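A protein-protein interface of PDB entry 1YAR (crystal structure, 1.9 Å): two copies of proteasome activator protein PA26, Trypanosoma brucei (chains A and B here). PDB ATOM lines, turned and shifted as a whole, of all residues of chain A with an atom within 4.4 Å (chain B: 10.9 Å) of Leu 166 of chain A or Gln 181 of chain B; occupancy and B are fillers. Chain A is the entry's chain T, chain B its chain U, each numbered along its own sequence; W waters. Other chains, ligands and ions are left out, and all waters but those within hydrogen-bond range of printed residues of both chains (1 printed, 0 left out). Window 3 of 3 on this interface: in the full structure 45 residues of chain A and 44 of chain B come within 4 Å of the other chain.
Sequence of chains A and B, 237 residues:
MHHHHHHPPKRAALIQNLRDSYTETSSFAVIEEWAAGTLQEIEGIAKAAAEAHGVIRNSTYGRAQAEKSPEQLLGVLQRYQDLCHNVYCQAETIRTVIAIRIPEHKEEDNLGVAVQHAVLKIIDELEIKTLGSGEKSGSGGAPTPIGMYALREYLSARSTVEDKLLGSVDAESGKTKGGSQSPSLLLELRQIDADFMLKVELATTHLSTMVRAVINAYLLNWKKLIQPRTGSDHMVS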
ATOM      1  N   ARG A  63     -20.565  23.790  16.469  1.00  0.00           N
ATOM      2  CA  ARG A  63     -21.688  23.107  15.822  1.00  0.00           C
ATOM      3  C   ARG A  63     -21.617  23.201  14.286  1.00  0.00           C
ATOM      4  O   ARG A  63     -22.058  22.296  13.586  1.00  0.00           O
ATOM      5  CB  ARG A  63     -23.021  23.661  16.361  1.00  0.00           C
ATOM      6  CG  ARG A  63     -24.239  22.757  16.158  1.00  0.00           C
ATOM      7  CD  ARG A  63     -25.525  23.283  16.838  1.00  0.00           C
ATOM      8  NE  ARG A  63     -26.739  22.577  16.413  1.00  0.00           N
ATOM      9  CZ  ARG A  63     -27.357  22.760  15.247  1.00  0.00           C
ATOM     10  NH1 ARG A  63     -26.877  23.614  14.352  1.00  0.00           N
ATOM     11  NH2 ARG A  63     -28.452  22.066  14.966  1.00  0.00           N
ATOM     12  N   ALA A  66     -20.264  20.276  12.408  1.00  0.00           N
ATOM     13  CA  ALA A  66     -21.160  19.135  12.275  1.00  0.00           C
ATOM     14  C   ALA A  66     -22.067  19.260  11.038  1.00  0.00           C
ATOM     15  O   ALA A  66     -22.718  18.299  10.643  1.00  0.00           O
ATOM     16  CB  ALA A  66     -21.992  18.966  13.531  1.00  0.00           C
ATOM     17  N   GLU A  67     -22.101  20.451  10.447  1.00  0.00           N
ATOM     18  CA  GLU A  67     -22.990  20.758   9.327  1.00  0.00           C
ATOM     19  C   GLU A  67     -22.340  20.504   7.971  1.00  0.00           C
ATOM     20  O   GLU A  67     -23.036  20.379   6.960  1.00  0.00           O
ATOM     21  CB  GLU A  67     -23.431  22.220   9.386  1.00  0.00           C
ATOM     22  CG  GLU A  67     -24.269  22.614  10.589  1.00  0.00           C
ATOM     23  CD  GLU A  67     -24.594  24.106  10.596  1.00  0.00           C
ATOM     24  OE1 GLU A  67     -25.089  24.605  11.627  1.00  0.00           O
ATOM     25  OE2 GLU A  67     -24.354  24.786   9.568  1.00  0.00           O
ATOM     26  N   GLU A 162     -22.366  13.709  14.359  1.00  0.00           N
ATOM     27  CA  GLU A 162     -23.142  14.769  13.710  1.00  0.00           C
ATOM     28  C   GLU A 162     -24.633  14.711  14.084  1.00  0.00           C
ATOM     29  O   GLU A 162     -25.204  15.723  14.535  1.00  0.00           O
ATOM     30  CB  GLU A 162     -22.966  14.731  12.192  1.00  0.00           C
ATOM     31  CG  GLU A 162     -21.597  15.149  11.682  1.00  0.00           C
ATOM     32  CD  GLU A 162     -21.369  14.702  10.240  1.00  0.00           C
ATOM     33  OE1 GLU A 162     -22.337  14.219   9.617  1.00  0.00           O
ATOM     34  OE2 GLU A 162     -20.241  14.859   9.722  1.00  0.00           O
ATOM     35  N   ASP A 163     -25.259  13.542  13.911  1.00  0.00           N
ATOM     36  CA  ASP A 163     -26.678  13.366  14.224  1.00  0.00           C
ATOM     37  C   ASP A 163     -26.991  13.773  15.673  1.00  0.00           C
ATOM     38  O   ASP A 163     -28.017  14.417  15.931  1.00  0.00           O
ATOM     39  CB  ASP A 163     -27.129  11.915  13.984  1.00  0.00           C
ATOM     40  CG  ASP A 163     -28.018  11.750  12.745  1.00  0.00           C
ATOM     41  OD1 ASP A 163     -28.817  12.670  12.442  1.00  0.00           O
ATOM     42  OD2 ASP A 163     -27.997  10.722  12.015  1.00  0.00           O
ATOM     43  N   LYS A 164     -26.116  13.402  16.608  1.00  0.00           N
ATOM     44  CA  LYS A 164     -26.325  13.705  18.032  1.00  0.00           C
ATOM     45  C   LYS A 164     -26.162  15.200  18.326  1.00  0.00           C
ATOM     46  O   LYS A 164     -26.906  15.766  19.142  1.00  0.00           O
ATOM     47  CB  LYS A 164     -25.377  12.891  18.919  1.00  0.00           C
ATOM     48  CG  LYS A 164     -25.654  11.418  18.960  1.00  0.00           C
ATOM     49  CD  LYS A 164     -24.798  10.714  20.009  1.00  0.00           C
ATOM     50  CE  LYS A 164     -24.879   9.207  19.836  1.00  0.00           C
ATOM     51  NZ  LYS A 164     -24.883   8.507  21.165  1.00  0.00           N
ATOM     52  N   LEU A 165     -25.197  15.824  17.654  1.00  0.00           N
ATOM     53  CA  LEU A 165     -24.908  17.253  17.796  1.00  0.00           C
ATOM     54  C   LEU A 165     -25.960  18.164  17.139  1.00  0.00           C
ATOM     55  O   LEU A 165     -26.238  19.262  17.630  1.00  0.00           O
ATOM     56  CB  LEU A 165     -23.519  17.587  17.230  1.00  0.00           C
ATOM     57  CG  LEU A 165     -22.297  17.162  18.057  1.00  0.00           C
ATOM     58  CD1 LEU A 165     -21.021  17.394  17.263  1.00  0.00           C
ATOM     59  CD2 LEU A 165     -22.255  17.933  19.401  1.00  0.00           C
ATOM     60  N   LEU A 166     -26.519  17.722  16.017  1.00  0.00           N
ATOM     61  CA  LEU A 166     -27.512  18.531  15.304  1.00  0.00           C
ATOM     62  C   LEU A 166     -28.912  18.275  15.853  1.00  0.00           C
ATOM     63  O   LEU A 166     -29.174  17.247  16.473  1.00  0.00           O
ATOM     64  CB  LEU A 166     -27.468  18.250  13.792  1.00  0.00           C
ATOM     65  CG  LEU A 166     -26.174  18.548  13.040  1.00  0.00           C
ATOM     66  CD1 LEU A 166     -26.175  17.866  11.671  1.00  0.00           C
ATOM     67  CD2 LEU A 166     -25.908  20.040  12.900  1.00  0.00           C
ATOM     68  N   GLY A 167     -29.828  19.202  15.619  1.00  0.00           N
ATOM     69  CA  GLY A 167     -31.245  18.880  15.852  1.00  0.00           C
ATOM     70  C   GLY A 167     -31.495  17.400  15.550  1.00  0.00           C
ATOM     71  O   GLY A 167     -31.787  16.608  16.448  1.00  0.00           O
ATOM     72  N   GLY A 179     -30.016  19.716  19.721  1.00  0.00           N
ATOM     73  CA  GLY A 179     -28.749  18.987  19.687  1.00  0.00           C
ATOM     74  C   GLY A 179     -28.153  18.749  21.065  1.00  0.00           C
ATOM     75  O   GLY A 179     -28.485  19.450  22.034  1.00  0.00           O
ATOM     76  N   GLY B  62     -27.898  13.398  -3.329  1.00  0.00           N
ATOM     77  CA  GLY B  62     -28.885  14.121  -2.532  1.00  0.00           C
ATOM     78  C   GLY B  62     -29.913  13.145  -2.013  1.00  0.00           C
ATOM     79  O   GLY B  62     -29.715  11.933  -2.078  1.00  0.00           O
ATOM     80  N   ARG B  63     -31.036  13.665  -1.526  1.00  0.00           N
ATOM     81  CA  ARG B  63     -32.088  12.825  -0.956  1.00  0.00           C
ATOM     82  C   ARG B  63     -32.663  11.850  -1.976  1.00  0.00           C
ATOM     83  O   ARG B  63     -33.090  10.751  -1.611  1.00  0.00           O
ATOM     84  CB  ARG B  63     -33.209  13.694  -0.359  1.00  0.00           C
ATOM     85  CG  ARG B  63     -34.343  12.907   0.322  1.00  0.00           C
ATOM     86  CD  ARG B  63     -35.561  13.774   0.685  1.00  0.00           C
ATOM     87  NE  ARG B  63     -36.702  12.984   1.140  1.00  0.00           N
ATOM     88  CZ  ARG B  63     -36.966  12.718   2.415  1.00  0.00           C
ATOM     89  NH1 ARG B  63     -36.163  13.172   3.373  1.00  0.00           N
ATOM     90  NH2 ARG B  63     -38.028  11.990   2.738  1.00  0.00           N
ATOM     91  N   VAL B 161     -29.441   3.148   6.030  1.00  0.00           N
ATOM     92  CA  VAL B 161     -29.070   4.522   5.776  1.00  0.00           C
ATOM     93  C   VAL B 161     -30.219   5.283   5.111  1.00  0.00           C
ATOM     94  O   VAL B 161     -30.511   6.421   5.474  1.00  0.00           O
ATOM     95  CB  VAL B 161     -27.750   4.591   4.976  1.00  0.00           C
ATOM     96  CG1 VAL B 161     -27.442   6.024   4.544  1.00  0.00           C
ATOM     97  CG2 VAL B 161     -26.599   4.034   5.838  1.00  0.00           C
ATOM     98  N   GLU B 162     -30.865   4.638   4.141  1.00  0.00           N
ATOM     99  CA  GLU B 162     -32.069   5.176   3.502  1.00  0.00           C
ATOM    100  C   GLU B 162     -33.116   5.585   4.526  1.00  0.00           C
ATOM    101  O   GLU B 162     -33.607   6.719   4.465  1.00  0.00           O
ATOM    102  CB  GLU B 162     -32.669   4.157   2.525  1.00  0.00           C
ATOM    103  CG  GLU B 162     -31.912   4.008   1.212  1.00  0.00           C
ATOM    104  CD  GLU B 162     -32.304   2.741   0.469  1.00  0.00           C
ATOM    105  OE1 GLU B 162     -33.323   2.102   0.845  1.00  0.00           O
ATOM    106  OE2 GLU B 162     -31.592   2.383  -0.490  1.00  0.00           O
ATOM    107  N   ASP B 163     -33.443   4.681   5.464  1.00  0.00           N
ATOM    108  CA  ASP B 163     -34.464   4.959   6.513  1.00  0.00           C
ATOM    109  C   ASP B 163     -34.131   6.187   7.367  1.00  0.00           C
ATOM    110  O   ASP B 163     -35.017   6.993   7.689  1.00  0.00           O
ATOM    111  CB  ASP B 163     -34.715   3.736   7.417  1.00  0.00           C
ATOM    112  CG  ASP B 163     -35.889   2.882   6.945  1.00  0.00           C
ATOM    113  OD1 ASP B 163     -36.756   3.414   6.201  1.00  0.00           O
ATOM    114  OD2 ASP B 163     -36.043   1.674   7.275  1.00  0.00           O
ATOM    115  N   LYS B 164     -32.855   6.341   7.707  1.00  0.00           N
ATOM    116  CA  LYS B 164     -32.393   7.488   8.486  1.00  0.00           C
ATOM    117  C   LYS B 164     -32.449   8.792   7.703  1.00  0.00           C
ATOM    118  O   LYS B 164     -32.778   9.836   8.272  1.00  0.00           O
ATOM    119  CB  LYS B 164     -30.969   7.273   8.991  1.00  0.00           C
ATOM    120  CG  LYS B 164     -30.861   6.248  10.103  1.00  0.00           C
ATOM    121  CD  LYS B 164     -29.404   5.985  10.485  1.00  0.00           C
ATOM    122  CE  LYS B 164     -29.310   4.774  11.412  1.00  0.00           C
ATOM    123  NZ  LYS B 164     -27.889   4.446  11.713  1.00  0.00           N
ATOM    124  N   LEU B 165     -32.116   8.729   6.414  1.00  0.00           N
ATOM    125  CA  LEU B 165     -32.133   9.892   5.542  1.00  0.00           C
ATOM    126  C   LEU B 165     -33.555  10.333   5.197  1.00  0.00           C
ATOM    127  O   LEU B 165     -33.818  11.526   5.051  1.00  0.00           O
ATOM    128  CB  LEU B 165     -31.332   9.631   4.252  1.00  0.00           C
ATOM    129  CG  LEU B 165     -29.796   9.638   4.316  1.00  0.00           C
ATOM    130  CD1 LEU B 165     -29.196   9.165   3.017  1.00  0.00           C
ATOM    131  CD2 LEU B 165     -29.246  11.019   4.676  1.00  0.00           C
ATOM    132  N   LEU B 166     -34.457   9.374   5.039  1.00  0.00           N
ATOM    133  CA  LEU B 166     -35.827   9.677   4.591  1.00  0.00           C
ATOM    134  C   LEU B 166     -36.713  10.077   5.756  1.00  0.00           C
ATOM    135  O   LEU B 166     -37.606  10.912   5.605  1.00  0.00           O
ATOM    136  CB  LEU B 166     -36.445   8.484   3.850  1.00  0.00           C
ATOM    137  CG  LEU B 166     -35.804   8.065   2.524  1.00  0.00           C
ATOM    138  CD1 LEU B 166     -36.423   6.745   2.036  1.00  0.00           C
ATOM    139  CD2 LEU B 166     -35.932   9.153   1.479  1.00  0.00           C
ATOM    140  N   GLY B 167     -36.458   9.482   6.916  1.00  0.00           N
ATOM    141  CA  GLY B 167     -37.278   9.697   8.103  1.00  0.00           C
ATOM    142  C   GLY B 167     -38.558   8.881   8.069  1.00  0.00           C
ATOM    143  O   GLY B 167     -39.291   8.815   9.070  1.00  0.00           O
ATOM    144  N   GLY B 178     -38.695  12.773  10.641  1.00  0.00           N
ATOM    145  CA  GLY B 178     -37.971  13.789   9.816  1.00  0.00           C
ATOM    146  C   GLY B 178     -36.577  13.292   9.477  1.00  0.00           C
ATOM    147  O   GLY B 178     -35.912  12.687  10.316  1.00  0.00           O
ATOM    148  N   GLY B 179     -36.128  13.553   8.251  1.00  0.00           N
ATOM    149  CA  GLY B 179     -34.853  13.010   7.775  1.00  0.00           C
ATOM    150  C   GLY B 179     -33.603  13.610   8.400  1.00  0.00           C
ATOM    151  O   GLY B 179     -33.531  14.817   8.643  1.00  0.00           O
ATOM    152  N   SER B 180     -32.607  12.757   8.648  1.00  0.00           N
ATOM    153  CA  SER B 180     -31.339  13.194   9.228  1.00  0.00           C
ATOM    154  C   SER B 180     -30.700  14.326   8.413  1.00  0.00           C
ATOM    155  O   SER B 180     -30.690  14.296   7.173  1.00  0.00           O
ATOM    156  CB  SER B 180     -30.380  12.002   9.353  1.00  0.00           C
ATOM    157  OG  SER B 180     -29.071  12.435   9.661  1.00  0.00           O
ATOM    158  N   GLN B 181     -30.161  15.317   9.115  1.00  0.00           N
ATOM    159  CA  GLN B 181     -29.416  16.402   8.471  1.00  0.00           C
ATOM    160  C   GLN B 181     -27.899  16.197   8.594  1.00  0.00           C
ATOM    161  O   GLN B 181     -27.122  17.124   8.357  1.00  0.00           O
ATOM    162  CB  GLN B 181     -29.811  17.785   9.031  1.00  0.00           C
ATOM    163  CG  GLN B 181     -31.285  18.204   8.780  1.00  0.00           C
ATOM    164  CD  GLN B 181     -31.694  18.123   7.311  1.00  0.00           C
ATOM    165  OE1 GLN B 181     -31.008  18.664   6.432  1.00  0.00           O
ATOM    166  NE2 GLN B 181     -32.813  17.439   7.042  1.00  0.00           N
ATOM    167  N   SER B 182     -27.488  14.980   8.947  1.00  0.00           N
ATOM    168  CA  SER B 182     -26.061  14.640   8.943  1.00  0.00           C
ATOM    169  C   SER B 182     -25.493  14.664   7.525  1.00  0.00           C
ATOM    170  O   SER B 182     -25.916  13.860   6.663  1.00  0.00           O
ATOM    171  CB  SER B 182     -25.828  13.261   9.566  1.00  0.00           C
ATOM    172  OG  SER B 182     -24.471  12.874   9.359  1.00  0.00           O
ATOM    173  N   PRO B 183     -24.525  15.546   7.278  1.00  0.00           N
ATOM    174  CA  PRO B 183     -23.863  15.617   5.970  1.00  0.00           C
ATOM    175  C   PRO B 183     -23.071  14.341   5.635  1.00  0.00           C
ATOM    176  O   PRO B 183     -23.062  13.903   4.478  1.00  0.00           O
ATOM    177  CB  PRO B 183     -22.922  16.825   6.109  1.00  0.00           C
ATOM    178  CG  PRO B 183     -22.730  17.012   7.576  1.00  0.00           C
ATOM    179  CD  PRO B 183     -23.982  16.549   8.222  1.00  0.00           C
ATOM    180  N   SER B 184     -22.438  13.743   6.646  1.00  0.00           N
ATOM    181  CA  SER B 184     -21.668  12.505   6.468  1.00  0.00           C
ATOM    182  C   SER B 184     -22.542  11.281   6.170  1.00  0.00           C
ATOM    183  O   SER B 184     -22.097  10.350   5.491  1.00  0.00           O
ATOM    184  CB  SER B 184     -20.761  12.271   7.694  1.00  0.00           C
ATOM    185  OG  SER B 184     -19.743  13.287   7.732  1.00  0.00           O
ATOM    186  N   LEU B 185     -23.777  11.281   6.674  1.00  0.00           N
ATOM    187  CA  LEU B 185     -24.709  10.189   6.403  1.00  0.00           C
ATOM    188  C   LEU B 185     -25.071  10.080   4.911  1.00  0.00           C
ATOM    189  O   LEU B 185     -25.234   8.974   4.386  1.00  0.00           O
ATOM    190  CB  LEU B 185     -25.983  10.317   7.237  1.00  0.00           C
ATOM    191  CG  LEU B 185     -26.959   9.128   7.161  1.00  0.00           C
ATOM    192  CD1 LEU B 185     -26.371   7.863   7.773  1.00  0.00           C
ATOM    193  CD2 LEU B 185     -28.289   9.467   7.847  1.00  0.00           C
ATOM    194  N   LEU B 186     -25.202  11.230   4.246  1.00  0.00           N
ATOM    195  CA  LEU B 186     -25.451  11.265   2.807  1.00  0.00           C
ATOM    196  C   LEU B 186     -24.230  10.773   2.038  1.00  0.00           C
ATOM    197  O   LEU B 186     -24.346   9.964   1.116  1.00  0.00           O
ATOM    198  CB  LEU B 186     -25.811  12.699   2.385  1.00  0.00           C
ATOM    199  CG  LEU B 186     -26.303  12.985   0.971  1.00  0.00           C
ATOM    200  CD1 LEU B 186     -27.498  12.087   0.592  1.00  0.00           C
ATOM    201  CD2 LEU B 186     -26.711  14.454   0.945  1.00  0.00           C
ATOM    202  N   LEU B 187     -23.048  11.256   2.414  1.00  0.00           N
ATOM    203  CA  LEU B 187     -21.811  10.726   1.841  1.00  0.00           C
ATOM    204  C   LEU B 187     -21.665   9.233   2.126  1.00  0.00           C
ATOM    205  O   LEU B 187     -21.086   8.515   1.324  1.00  0.00           O
ATOM    206  CB  LEU B 187     -20.583  11.486   2.332  1.00  0.00           C
ATOM    207  CG  LEU B 187     -20.506  12.966   1.940  1.00  0.00           C
ATOM    208  CD1 LEU B 187     -19.455  13.678   2.786  1.00  0.00           C
ATOM    209  CD2 LEU B 187     -20.196  13.115   0.454  1.00  0.00           C
ATOM    210  N   GLU B 188     -22.188   8.774   3.256  1.00  0.00           N
ATOM    211  CA  GLU B 188     -22.095   7.347   3.581  1.00  0.00           C
ATOM    212  C   GLU B 188     -22.999   6.499   2.690  1.00  0.00           C
ATOM    213  O   GLU B 188     -22.656   5.362   2.384  1.00  0.00           O
ATOM    214  CB  GLU B 188     -22.389   7.044   5.049  1.00  0.00           C
ATOM    215  CG  GLU B 188     -22.040   5.591   5.403  1.00  0.00           C
ATOM    216  CD  GLU B 188     -22.569   5.132   6.747  1.00  0.00           C
ATOM    217  OE1 GLU B 188     -22.429   3.919   7.038  1.00  0.00           O
ATOM    218  OE2 GLU B 188     -23.120   5.955   7.509  1.00  0.00           O
HETATM  219  O   HOH W   1     -29.518  15.183  12.121  1.00  0.00           O
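Among the printed residues, merely in contact across the chains: Ala 66 of chain A with Pro 183 of chain B (3.2 Å), Glu 67 of chain A with Pro 183 of chain B (3.4 Å) and Leu 166 of chain A with Gln 181 of chain B (3.5 Å).
Of chain B, only Gln 181 comes within 4 Å of Leu 166 of chain A.
Ala 66 of chain A touches just one residue of chain B: Pro 183 (3.2 Å).
No residue of chain B comes within 4 Å of Gly 179 of chain A.
Of the printed residues of chain B, Glu 162 of chain A touches Ser 182, Pro 183 and Ser 184.
Of the printed residues of chain A, Ser 184 of chain B touches Glu 162.
Of the printed residues of chain A, Pro 183 of chain B touches Ala 66, Glu 67 and Glu 162.
Of the printed residues of chain A, Ser 180 of chain B touches Asp 163 (2.8 Å).
Of the printed residues of chain A, Ser 182 of chain B touches Glu 162.
The nearest printed residue of chain A that does not touch Pro 183 of chain B is Leu 166 of chain A (4.3 Å).
Hydrophobic or aromatic side chains of chain A within 4 Å of the printed part of chain B: Leu 166.
Of the 20 printed residues of chain B, 5 touch a printed residue of chain A.
Printed residues of chain B that touch a printed residue of chain A: Ser 180, Gln 181, Ser 182, Pro 183 and Ser 184.
Hydrophobic or aromatic side chains of chain B within 4 Å of the printed part of chain A: Pro 183.
Among the printed residues, 7 pairs touch across the chains.
Among the printed residues, no Asp or Glu carboxylate lies within 4 Å of a Lys or Arg side-chain nitrogen of the other chain.
Positions printed for both chains: 63, 162, 163, 164, 165, 166, 167 and 179.
Of the 7 pairs that touch across the chains among the printed residues, none has its exchanged pair printed and touching as well.
The side-chain hydroxyl (OG) of Ser 182 of chain B is in hydrogen-bond range of the side-chain carboxylate (OE1) of Glu 162 of chain A, 2.5 Å away.
OE2 of Glu 162 of chain A lies within hydrogen-bond range of OG of Ser 184 of chain B, 2.6 Å away.
OD1 of Asp 163 of chain A sits at hydrogen-bond distance from OG of Ser 180 of chain B, 2.8 Å away.
OE1 of Glu 162 of chain A sits close to N of Pro 183 of chain B.
The guanidinium group (NH1) of Arg 63 of chain A is in salt-bridge range of the side-chain carboxylate (OE1) of Glu 67 of chain A, 3.4 Å away.
The backbone carbonyl oxygen (O) of Lys 164 of chain B is in hydrogen-bond range of the backbone NH (N) of Ser 180 of chain B, at 3.0 Å.
NE2 of Gln 181 of chain B sits at hydrogen-bond distance from O of Gly 179 of chain B.
The side-chain hydroxyl (OG) of Ser 180 of chain B sits at hydrogen-bond distance from the backbone NH (N) of Ser 182 of chain B (3.1 Å).
OG of Ser 182 of chain B lies close to N of Ser 184 of chain B.
The side-chain hydroxyl (OG) of Ser 182 of chain B is in hydrogen-bond range of the backbone NH (N) of Leu 185 of chain B (3.2 Å).
Water W1 lies within hydrogen-bond range of OD1 of Asp 163 of chain A (2.6 Å) and N of Gln 181 of chain B (3.1 Å).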
